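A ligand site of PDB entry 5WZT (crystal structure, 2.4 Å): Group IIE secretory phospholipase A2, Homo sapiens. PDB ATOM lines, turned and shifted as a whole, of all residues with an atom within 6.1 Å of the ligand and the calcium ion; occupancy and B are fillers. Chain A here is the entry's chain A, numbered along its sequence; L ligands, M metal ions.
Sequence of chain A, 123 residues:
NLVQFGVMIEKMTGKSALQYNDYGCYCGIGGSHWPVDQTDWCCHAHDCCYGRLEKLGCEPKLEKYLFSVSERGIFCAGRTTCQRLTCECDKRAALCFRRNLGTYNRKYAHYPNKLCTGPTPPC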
ATOM      1  N   LEU A   2       6.007  24.869  -4.825  1.00  0.00           N
ATOM      2  CA  LEU A   2       7.052  25.609  -4.097  1.00  0.00           C
ATOM      3  C   LEU A   2       6.705  27.055  -3.724  1.00  0.00           C
ATOM      4  O   LEU A   2       7.568  27.778  -3.190  1.00  0.00           O
ATOM      5  CB  LEU A   2       8.361  25.587  -4.917  1.00  0.00           C
ATOM      6  CG  LEU A   2       9.146  24.274  -4.980  1.00  0.00           C
ATOM      7  CD1 LEU A   2      10.285  24.376  -5.988  1.00  0.00           C
ATOM      8  CD2 LEU A   2       9.688  23.880  -3.599  1.00  0.00           C
ATOM      9  N   VAL A   3       5.470  27.485  -3.963  1.00  0.00           N
ATOM     10  CA  VAL A   3       5.092  28.904  -3.792  1.00  0.00           C
ATOM     11  C   VAL A   3       5.256  29.417  -2.337  1.00  0.00           C
ATOM     12  O   VAL A   3       6.003  30.366  -2.108  1.00  0.00           O
ATOM     13  CB  VAL A   3       3.685  29.220  -4.388  1.00  0.00           C
ATOM     14  CG1 VAL A   3       2.546  28.479  -3.673  1.00  0.00           C
ATOM     15  CG2 VAL A   3       3.416  30.729  -4.412  1.00  0.00           C
ATOM     16  N   PHE A   5       6.809  28.165   0.318  1.00  0.00           N
ATOM     17  CA  PHE A   5       8.190  28.080   0.798  1.00  0.00           C
ATOM     18  C   PHE A   5       9.069  29.234   0.288  1.00  0.00           C
ATOM     19  O   PHE A   5       9.750  29.912   1.065  1.00  0.00           O
ATOM     20  CB  PHE A   5       8.784  26.727   0.406  1.00  0.00           C
ATOM     21  CG  PHE A   5      10.134  26.439   1.006  1.00  0.00           C
ATOM     22  CD1 PHE A   5      10.494  26.878   2.292  1.00  0.00           C
ATOM     23  CD2 PHE A   5      11.054  25.686   0.288  1.00  0.00           C
ATOM     24  CE1 PHE A   5      11.751  26.593   2.814  1.00  0.00           C
ATOM     25  CE2 PHE A   5      12.311  25.402   0.810  1.00  0.00           C
ATOM     26  CZ  PHE A   5      12.656  25.848   2.074  1.00  0.00           C
ATOM     27  N   GLY A   6       9.007  29.443  -1.039  1.00  0.00           N
ATOM     28  CA  GLY A   6       9.667  30.558  -1.681  1.00  0.00           C
ATOM     29  C   GLY A   6       9.267  31.875  -1.077  1.00  0.00           C
ATOM     30  O   GLY A   6      10.124  32.749  -0.868  1.00  0.00           O
ATOM     31  N   VAL A   7       7.972  32.027  -0.747  1.00  0.00           N
ATOM     32  CA  VAL A   7       7.542  33.252  -0.075  1.00  0.00           C
ATOM     33  C   VAL A   7       8.188  33.355   1.310  1.00  0.00           C
ATOM     34  O   VAL A   7       8.711  34.407   1.683  1.00  0.00           O
ATOM     35  CB  VAL A   7       6.001  33.382   0.033  1.00  0.00           C
ATOM     36  CG1 VAL A   7       5.593  34.598   0.883  1.00  0.00           C
ATOM     37  CG2 VAL A   7       5.378  33.507  -1.351  1.00  0.00           C
ATOM     38  N   ILE A   9      10.937  32.005   2.360  1.00  0.00           N
ATOM     39  CA  ILE A   9      12.365  32.296   2.174  1.00  0.00           C
ATOM     40  C   ILE A   9      12.610  33.794   1.947  1.00  0.00           C
ATOM     41  O   ILE A   9      13.508  34.373   2.568  1.00  0.00           O
ATOM     42  CB  ILE A   9      12.995  31.455   1.053  1.00  0.00           C
ATOM     43  CG1 ILE A   9      13.001  29.972   1.451  1.00  0.00           C
ATOM     44  CG2 ILE A   9      14.436  31.895   0.793  1.00  0.00           C
ATOM     45  CD1 ILE A   9      13.009  29.029   0.274  1.00  0.00           C
ATOM     46  N   ALA A  17      13.898  33.470  -3.537  1.00  0.00           N
ATOM     47  CA  ALA A  17      14.052  32.025  -3.368  1.00  0.00           C
ATOM     48  C   ALA A  17      14.964  31.370  -4.421  1.00  0.00           C
ATOM     49  O   ALA A  17      15.611  30.351  -4.147  1.00  0.00           O
ATOM     50  CB  ALA A  17      12.695  31.355  -3.397  1.00  0.00           C
ATOM     51  N   LEU A  18      15.006  31.950  -5.619  1.00  0.00           N
ATOM     52  CA  LEU A  18      15.899  31.501  -6.695  1.00  0.00           C
ATOM     53  C   LEU A  18      17.377  31.482  -6.284  1.00  0.00           C
ATOM     54  O   LEU A  18      18.150  30.674  -6.806  1.00  0.00           O
ATOM     55  CB  LEU A  18      15.740  32.381  -7.946  1.00  0.00           C
ATOM     56  CG  LEU A  18      14.353  32.499  -8.598  1.00  0.00           C
ATOM     57  CD1 LEU A  18      14.463  33.380  -9.836  1.00  0.00           C
ATOM     58  CD2 LEU A  18      13.776  31.131  -8.937  1.00  0.00           C
ATOM     59  N   TYR A  20      18.497  30.442  -3.537  1.00  0.00           N
ATOM     60  CA  TYR A  20      18.680  29.175  -2.836  1.00  0.00           C
ATOM     61  C   TYR A  20      18.314  27.965  -3.700  1.00  0.00           C
ATOM     62  O   TYR A  20      18.208  26.860  -3.192  1.00  0.00           O
ATOM     63  CB  TYR A  20      17.854  29.174  -1.544  1.00  0.00           C
ATOM     64  CG  TYR A  20      18.325  30.189  -0.525  1.00  0.00           C
ATOM     65  CD1 TYR A  20      17.933  31.534  -0.594  1.00  0.00           C
ATOM     66  CD2 TYR A  20      19.168  29.796   0.517  1.00  0.00           C
ATOM     67  CE1 TYR A  20      18.367  32.452   0.346  1.00  0.00           C
ATOM     68  CE2 TYR A  20      19.613  30.720   1.451  1.00  0.00           C
ATOM     69  CZ  TYR A  20      19.219  32.038   1.366  1.00  0.00           C
ATOM     70  OH  TYR A  20      19.656  32.934   2.305  1.00  0.00           O
ATOM     71  N   ASN A  21      18.129  28.157  -4.994  1.00  0.00           N
ATOM     72  CA  ASN A  21      17.828  27.039  -5.906  1.00  0.00           C
ATOM     73  C   ASN A  21      19.152  26.674  -6.561  1.00  0.00           C
ATOM     74  O   ASN A  21      19.940  27.565  -6.940  1.00  0.00           O
ATOM     75  CB  ASN A  21      16.754  27.458  -6.924  1.00  0.00           C
ATOM     76  CG  ASN A  21      16.271  26.310  -7.812  1.00  0.00           C
ATOM     77  OD1 ASN A  21      16.238  26.461  -9.037  1.00  0.00           O
ATOM     78  ND2 ASN A  21      15.881  25.171  -7.220  1.00  0.00           N
ATOM     79  N   ASP A  22      19.425  25.367  -6.603  1.00  0.00           N
ATOM     80  CA  ASP A  22      20.728  24.808  -7.000  1.00  0.00           C
ATOM     81  C   ASP A  22      21.899  25.317  -6.170  1.00  0.00           C
ATOM     82  O   ASP A  22      23.050  25.126  -6.567  1.00  0.00           O
ATOM     83  CB  ASP A  22      21.006  25.039  -8.488  1.00  0.00           C
ATOM     84  CG  ASP A  22      19.929  24.504  -9.373  1.00  0.00           C
ATOM     85  OD1 ASP A  22      19.248  23.536  -8.968  1.00  0.00           O
ATOM     86  OD2 ASP A  22      19.752  25.068 -10.463  1.00  0.00           O
ATOM     87  N   CYS A  25      25.370  21.796  -2.813  1.00  0.00           N
ATOM     88  CA  CYS A  25      25.141  20.408  -3.146  1.00  0.00           C
ATOM     89  C   CYS A  25      23.780  19.875  -2.759  1.00  0.00           C
ATOM     90  O   CYS A  25      23.396  18.812  -3.276  1.00  0.00           O
ATOM     91  CB  CYS A  25      26.276  19.575  -2.544  1.00  0.00           C
ATOM     92  SG  CYS A  25      27.864  19.912  -3.357  1.00  0.00           S
ATOM     93  N   TYR A  26      23.026  20.610  -1.920  1.00  0.00           N
ATOM     94  CA  TYR A  26      21.731  20.154  -1.400  1.00  0.00           C
ATOM     95  C   TYR A  26      20.476  20.998  -1.677  1.00  0.00           C
ATOM     96  O   TYR A  26      19.380  20.460  -1.615  1.00  0.00           O
ATOM     97  CB  TYR A  26      21.834  19.843   0.113  1.00  0.00           C
ATOM     98  CG  TYR A  26      22.506  18.530   0.357  1.00  0.00           C
ATOM     99  CD1 TYR A  26      21.775  17.339   0.389  1.00  0.00           C
ATOM    100  CD2 TYR A  26      23.891  18.447   0.470  1.00  0.00           C
ATOM    101  CE1 TYR A  26      22.403  16.109   0.567  1.00  0.00           C
ATOM    102  CE2 TYR A  26      24.529  17.231   0.647  1.00  0.00           C
ATOM    103  CZ  TYR A  26      23.781  16.065   0.690  1.00  0.00           C
ATOM    104  OH  TYR A  26      24.401  14.852   0.853  1.00  0.00           O
ATOM    105  N   CYS A  27      20.608  22.284  -1.963  1.00  0.00           N
ATOM    106  CA  CYS A  27      19.414  23.111  -2.153  1.00  0.00           C
ATOM    107  C   CYS A  27      18.928  22.968  -3.598  1.00  0.00           C
ATOM    108  O   CYS A  27      19.681  23.244  -4.549  1.00  0.00           O
ATOM    109  CB  CYS A  27      19.690  24.564  -1.829  1.00  0.00           C
ATOM    110  SG  CYS A  27      20.510  24.852  -0.259  1.00  0.00           S
ATOM    111  N   GLY A  28      17.668  22.555  -3.746  1.00  0.00           N
ATOM    112  CA  GLY A  28      17.106  22.171  -5.044  1.00  0.00           C
ATOM    113  C   GLY A  28      16.805  20.695  -4.995  1.00  0.00           C
ATOM    114  O   GLY A  28      17.116  20.058  -4.003  1.00  0.00           O
ATOM    115  N   ILE A  29      16.201  20.142  -6.048  1.00  0.00           N
ATOM    116  CA  ILE A  29      15.765  18.750  -5.966  1.00  0.00           C
ATOM    117  C   ILE A  29      16.940  17.779  -5.759  1.00  0.00           C
ATOM    118  O   ILE A  29      18.033  17.979  -6.301  1.00  0.00           O
ATOM    119  CB  ILE A  29      14.864  18.305  -7.161  1.00  0.00           C
ATOM    120  CG1 ILE A  29      15.592  18.422  -8.524  1.00  0.00           C
ATOM    121  CG2 ILE A  29      13.536  19.078  -7.128  1.00  0.00           C
ATOM    122  CD1 ILE A  29      15.846  17.074  -9.192  1.00  0.00           C
ATOM    123  N   GLY A  30      16.710  16.770  -4.910  1.00  0.00           N
ATOM    124  CA  GLY A  30      17.724  15.799  -4.549  1.00  0.00           C
ATOM    125  C   GLY A  30      18.872  16.388  -3.748  1.00  0.00           C
ATOM    126  O   GLY A  30      18.688  17.317  -2.962  1.00  0.00           O
ATOM    127  N   GLY A  31      20.064  15.860  -3.959  1.00  0.00           N
ATOM    128  CA  GLY A  31      21.243  16.303  -3.239  1.00  0.00           C
ATOM    129  C   GLY A  31      22.055  15.107  -2.809  1.00  0.00           C
ATOM    130  O   GLY A  31      21.507  14.033  -2.594  1.00  0.00           O
ATOM    131  N   CYS A  42      21.467  23.591   5.986  1.00  0.00           N
ATOM    132  CA  CYS A  42      20.042  23.866   6.171  1.00  0.00           C
ATOM    133  C   CYS A  42      19.237  23.014   5.214  1.00  0.00           C
ATOM    134  O   CYS A  42      18.267  22.389   5.632  1.00  0.00           O
ATOM    135  CB  CYS A  42      19.671  25.336   5.946  1.00  0.00           C
ATOM    136  SG  CYS A  42      20.629  26.559   6.864  1.00  0.00           S
ATOM    137  N   CYS A  43      19.658  22.985   3.956  1.00  0.00           N
ATOM    138  CA  CYS A  43      18.989  22.201   2.903  1.00  0.00           C
ATOM    139  C   CYS A  43      19.093  20.700   3.086  1.00  0.00           C
ATOM    140  O   CYS A  43      18.127  19.989   2.822  1.00  0.00           O
ATOM    141  CB  CYS A  43      19.514  22.581   1.512  1.00  0.00           C
ATOM    142  SG  CYS A  43      19.117  24.277   1.096  1.00  0.00           S
ATOM    143  N   HIS A  44      20.269  20.209   3.513  1.00  0.00           N
ATOM    144  CA  HIS A  44      20.431  18.801   3.920  1.00  0.00           C
ATOM    145  C   HIS A  44      19.464  18.443   5.060  1.00  0.00           C
ATOM    146  O   HIS A  44      18.744  17.434   4.979  1.00  0.00           O
ATOM    147  CB  HIS A  44      21.889  18.517   4.333  1.00  0.00           C
ATOM    148  CG  HIS A  44      22.121  17.154   4.913  1.00  0.00           C
ATOM    149  ND1 HIS A  44      21.907  16.860   6.247  1.00  0.00           N
ATOM    150  CD2 HIS A  44      22.592  16.012   4.348  1.00  0.00           C
ATOM    151  CE1 HIS A  44      22.203  15.596   6.462  1.00  0.00           C
ATOM    152  NE2 HIS A  44      22.620  15.051   5.331  1.00  0.00           N
ATOM    153  N   HIS A  46      16.722  20.079   5.733  1.00  0.00           N
ATOM    154  CA  HIS A  46      15.377  20.210   5.146  1.00  0.00           C
ATOM    155  C   HIS A  46      14.974  18.965   4.349  1.00  0.00           C
ATOM    156  O   HIS A  46      13.870  18.453   4.532  1.00  0.00           O
ATOM    157  CB  HIS A  46      15.296  21.465   4.283  1.00  0.00           C
ATOM    158  CG  HIS A  46      13.917  21.772   3.807  1.00  0.00           C
ATOM    159  ND1 HIS A  46      13.451  21.394   2.569  1.00  0.00           N
ATOM    160  CD2 HIS A  46      12.890  22.420   4.402  1.00  0.00           C
ATOM    161  CE1 HIS A  46      12.205  21.796   2.419  1.00  0.00           C
ATOM    162  NE2 HIS A  46      11.837  22.412   3.533  1.00  0.00           N
ATOM    163  N   ASP A  47      15.861  18.466   3.491  1.00  0.00           N
ATOM    164  CA  ASP A  47      15.695  17.148   2.845  1.00  0.00           C
ATOM    165  C   ASP A  47      15.367  16.020   3.862  1.00  0.00           C
ATOM    166  O   ASP A  47      14.447  15.204   3.663  1.00  0.00           O
ATOM    167  CB  ASP A  47      16.973  16.739   2.118  1.00  0.00           C
ATOM    168  CG  ASP A  47      17.212  17.483   0.789  1.00  0.00           C
ATOM    169  OD1 ASP A  47      16.439  18.359   0.364  1.00  0.00           O
ATOM    170  OD2 ASP A  47      18.215  17.136   0.145  1.00  0.00           O
ATOM    171  N   TYR A  50      11.841  16.470   5.200  1.00  0.00           N
ATOM    172  CA  TYR A  50      10.869  15.948   4.240  1.00  0.00           C
ATOM    173  C   TYR A  50      10.819  14.413   4.250  1.00  0.00           C
ATOM    174  O   TYR A  50       9.743  13.831   4.230  1.00  0.00           O
ATOM    175  CB  TYR A  50      11.086  16.552   2.833  1.00  0.00           C
ATOM    176  CG  TYR A  50      10.382  17.896   2.577  1.00  0.00           C
ATOM    177  CD1 TYR A  50      10.038  18.762   3.610  1.00  0.00           C
ATOM    178  CD2 TYR A  50      10.089  18.327   1.261  1.00  0.00           C
ATOM    179  CE1 TYR A  50       9.392  19.984   3.351  1.00  0.00           C
ATOM    180  CE2 TYR A  50       9.467  19.547   0.996  1.00  0.00           C
ATOM    181  CZ  TYR A  50       9.123  20.386   2.036  1.00  0.00           C
ATOM    182  OH  TYR A  50       8.474  21.598   1.795  1.00  0.00           O
ATOM    183  N   LYS A  61       6.257  17.625  -0.501  1.00  0.00           N
ATOM    184  CA  LYS A  61       6.476  18.288  -1.800  1.00  0.00           C
ATOM    185  C   LYS A  61       5.236  18.981  -2.308  1.00  0.00           C
ATOM    186  O   LYS A  61       5.345  19.942  -3.046  1.00  0.00           O
ATOM    187  CB  LYS A  61       6.970  17.290  -2.856  1.00  0.00           C
ATOM    188  CG  LYS A  61       8.472  17.066  -2.790  1.00  0.00           C
ATOM    189  CD  LYS A  61       8.895  15.699  -3.312  1.00  0.00           C
ATOM    190  CE  LYS A  61      10.418  15.624  -3.379  1.00  0.00           C
ATOM    191  NZ  LYS A  61      10.890  14.237  -3.104  1.00  0.00           N
ATOM    192  N   ALA A  93      14.010  25.625   8.024  1.00  0.00           N
ATOM    193  CA  ALA A  93      14.917  25.906   6.907  1.00  0.00           C
ATOM    194  C   ALA A  93      15.085  27.414   6.621  1.00  0.00           C
ATOM    195  O   ALA A  93      16.194  27.884   6.367  1.00  0.00           O
ATOM    196  CB  ALA A  93      14.460  25.164   5.653  1.00  0.00           C
ATOM    197  N   PHE A  97      18.357  29.592   6.989  1.00  0.00           N
ATOM    198  CA  PHE A  97      18.902  30.458   5.921  1.00  0.00           C
ATOM    199  C   PHE A  97      19.185  31.884   6.409  1.00  0.00           C
ATOM    200  O   PHE A  97      20.281  32.392   6.186  1.00  0.00           O
ATOM    201  CB  PHE A  97      17.979  30.572   4.702  1.00  0.00           C
ATOM    202  CG  PHE A  97      17.756  29.296   3.950  1.00  0.00           C
ATOM    203  CD1 PHE A  97      18.781  28.351   3.770  1.00  0.00           C
ATOM    204  CD2 PHE A  97      16.528  29.078   3.331  1.00  0.00           C
ATOM    205  CE1 PHE A  97      18.549  27.196   3.029  1.00  0.00           C
ATOM    206  CE2 PHE A  97      16.290  27.931   2.571  1.00  0.00           C
ATOM    207  CZ  PHE A  97      17.319  26.986   2.415  1.00  0.00           C
HETATM  208  O1  LIG L   1      14.406  18.306  -2.737  1.00  0.00           O
HETATM  209  C1  LIG L   1      13.378  18.476  -2.040  1.00  0.00           C
HETATM  210  O2  LIG L   1      12.684  17.561  -1.547  1.00  0.00           O
HETATM  211  C2  LIG L   1      12.948  19.935  -1.714  1.00  0.00           C
HETATM  212  O3  LIG L   1      14.037  20.888  -1.894  1.00  0.00           O
HETATM  213  C3  LIG L   1      13.934  21.904  -2.825  1.00  0.00           C
HETATM  214  C4  LIG L   1      13.389  21.638  -4.094  1.00  0.00           C
HETATM  215  C5  LIG L   1      13.303  22.651  -5.011  1.00  0.00           C
HETATM  216  C6  LIG L   1      13.781  23.904  -4.644  1.00  0.00           C
HETATM  217  C7  LIG L   1      14.293  24.132  -3.428  1.00  0.00           C
HETATM  218  C8  LIG L   1      14.384  23.151  -2.504  1.00  0.00           C
HETATM  219  C9  LIG L   1      14.974  23.728  -1.415  1.00  0.00           C
HETATM  220  C10 LIG L   1      15.286  23.143  -0.237  1.00  0.00           C
HETATM  221  O4  LIG L   1      14.908  23.541   0.861  1.00  0.00           O
HETATM  222  C11 LIG L   1      16.223  21.942  -0.295  1.00  0.00           C
HETATM  223  O5  LIG L   1      16.674  21.530  -1.350  1.00  0.00           O
HETATM  224  N1  LIG L   1      16.423  21.334   0.845  1.00  0.00           N
HETATM  225  C12 LIG L   1      15.207  25.008  -1.682  1.00  0.00           C
HETATM  226  C13 LIG L   1      15.840  25.998  -0.703  1.00  0.00           C
HETATM  227  N2  LIG L   1      14.797  25.271  -2.923  1.00  0.00           N
HETATM  228  C14 LIG L   1      14.826  26.601  -3.692  1.00  0.00           C
HETATM  229  C15 LIG L   1      13.515  27.160  -3.798  1.00  0.00           C
HETATM  230  C16 LIG L   1      13.127  27.874  -4.950  1.00  0.00           C
HETATM  231  C17 LIG L   1      11.837  28.427  -5.055  1.00  0.00           C
HETATM  232 BR1  LIG L   1      11.278  29.407  -6.595  1.00  0.00          BR
HETATM  233  C18 LIG L   1      10.923  28.252  -4.030  1.00  0.00           C
HETATM  234  C19 LIG L   1      11.284  27.539  -2.894  1.00  0.00           C
HETATM  235  C20 LIG L   1      12.567  26.998  -2.772  1.00  0.00           C
HETATM  236 CA    CA M   1      17.498  19.261  -1.879  1.00  0.00          CA
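An oxygen (O5) of the ligand sits close to the backbone NH (N) of Gly 28.
O of Cys 43 lies within hydrogen-bond range of N1 of the ligand (2.9 Å).
An oxygen (O4) of the ligand sits at hydrogen-bond distance from a ring nitrogen (ND1) of His 46, at 3.1 Å.
Along chain A the residues within 4 Å of the calcium ion span positions 26 to 47.
The nearest printed residue that does not touch the calcium ion is Ile 29 (4.2 Å).
The calcium ion is bound by O of Tyr 26 (2.2 Å), O of Gly 28 (2.3 Å), O5 of the ligand (2.5 Å), O of Gly 30 (2.5 Å) and OD1 of Asp 47 (2.6 Å).
Slightly farther from the calcium ion lies the side-chain carboxylate (OD2) of Asp 47 (3.0 Å).
SG of Cys 43 forms a disulfide with SG of Cys 27 (2.0 Å).
The backbone carbonyl oxygen (O) of Cys 27 sits at hydrogen-bond distance from the backbone NH (N) of Asp 22, 3.0 Å away.
N of Phe 97 is in hydrogen-bond range of SG of Cys 42 (3.8 Å).
Leu 2 touches the ligand.
CE2 of Phe 5 touches O4 of the ligand (3.2 Å).
Gly 6 touches the ligand.
Ile 9 touches the ligand.
Ala 17 touches the ligand (CB to C17, 3.5 Å).
Leu 18 touches the ligand.
O of Tyr 20 touches C14 of the ligand, at 3.4 Å.
Asn 21 touches the ligand (ND2 to C6, 3.6 Å).
CA of Cys 27 touches O5 of the ligand, at 3.3 Å.
Ile 29 touches the ligand (CA to O1, 3.5 Å).
CD2 of Tyr 50 touches O2 of the ligand, at 3.9 Å.
Lys 61 touches the ligand.
Phe 97 touches the ligand.
Hydrophobic or aromatic side chains within 4 Å of the ligand: Leu 2, Phe 5, Ile 9, Ala 17, Leu 18, Tyr 20, Ile 29, His 46, Tyr 50 and Phe 97.
Of the 27 residues printed, 19 come within 4 Å of the ligand.
Along chain A the residues within 4 Å of the ligand span positions 2 to 97.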
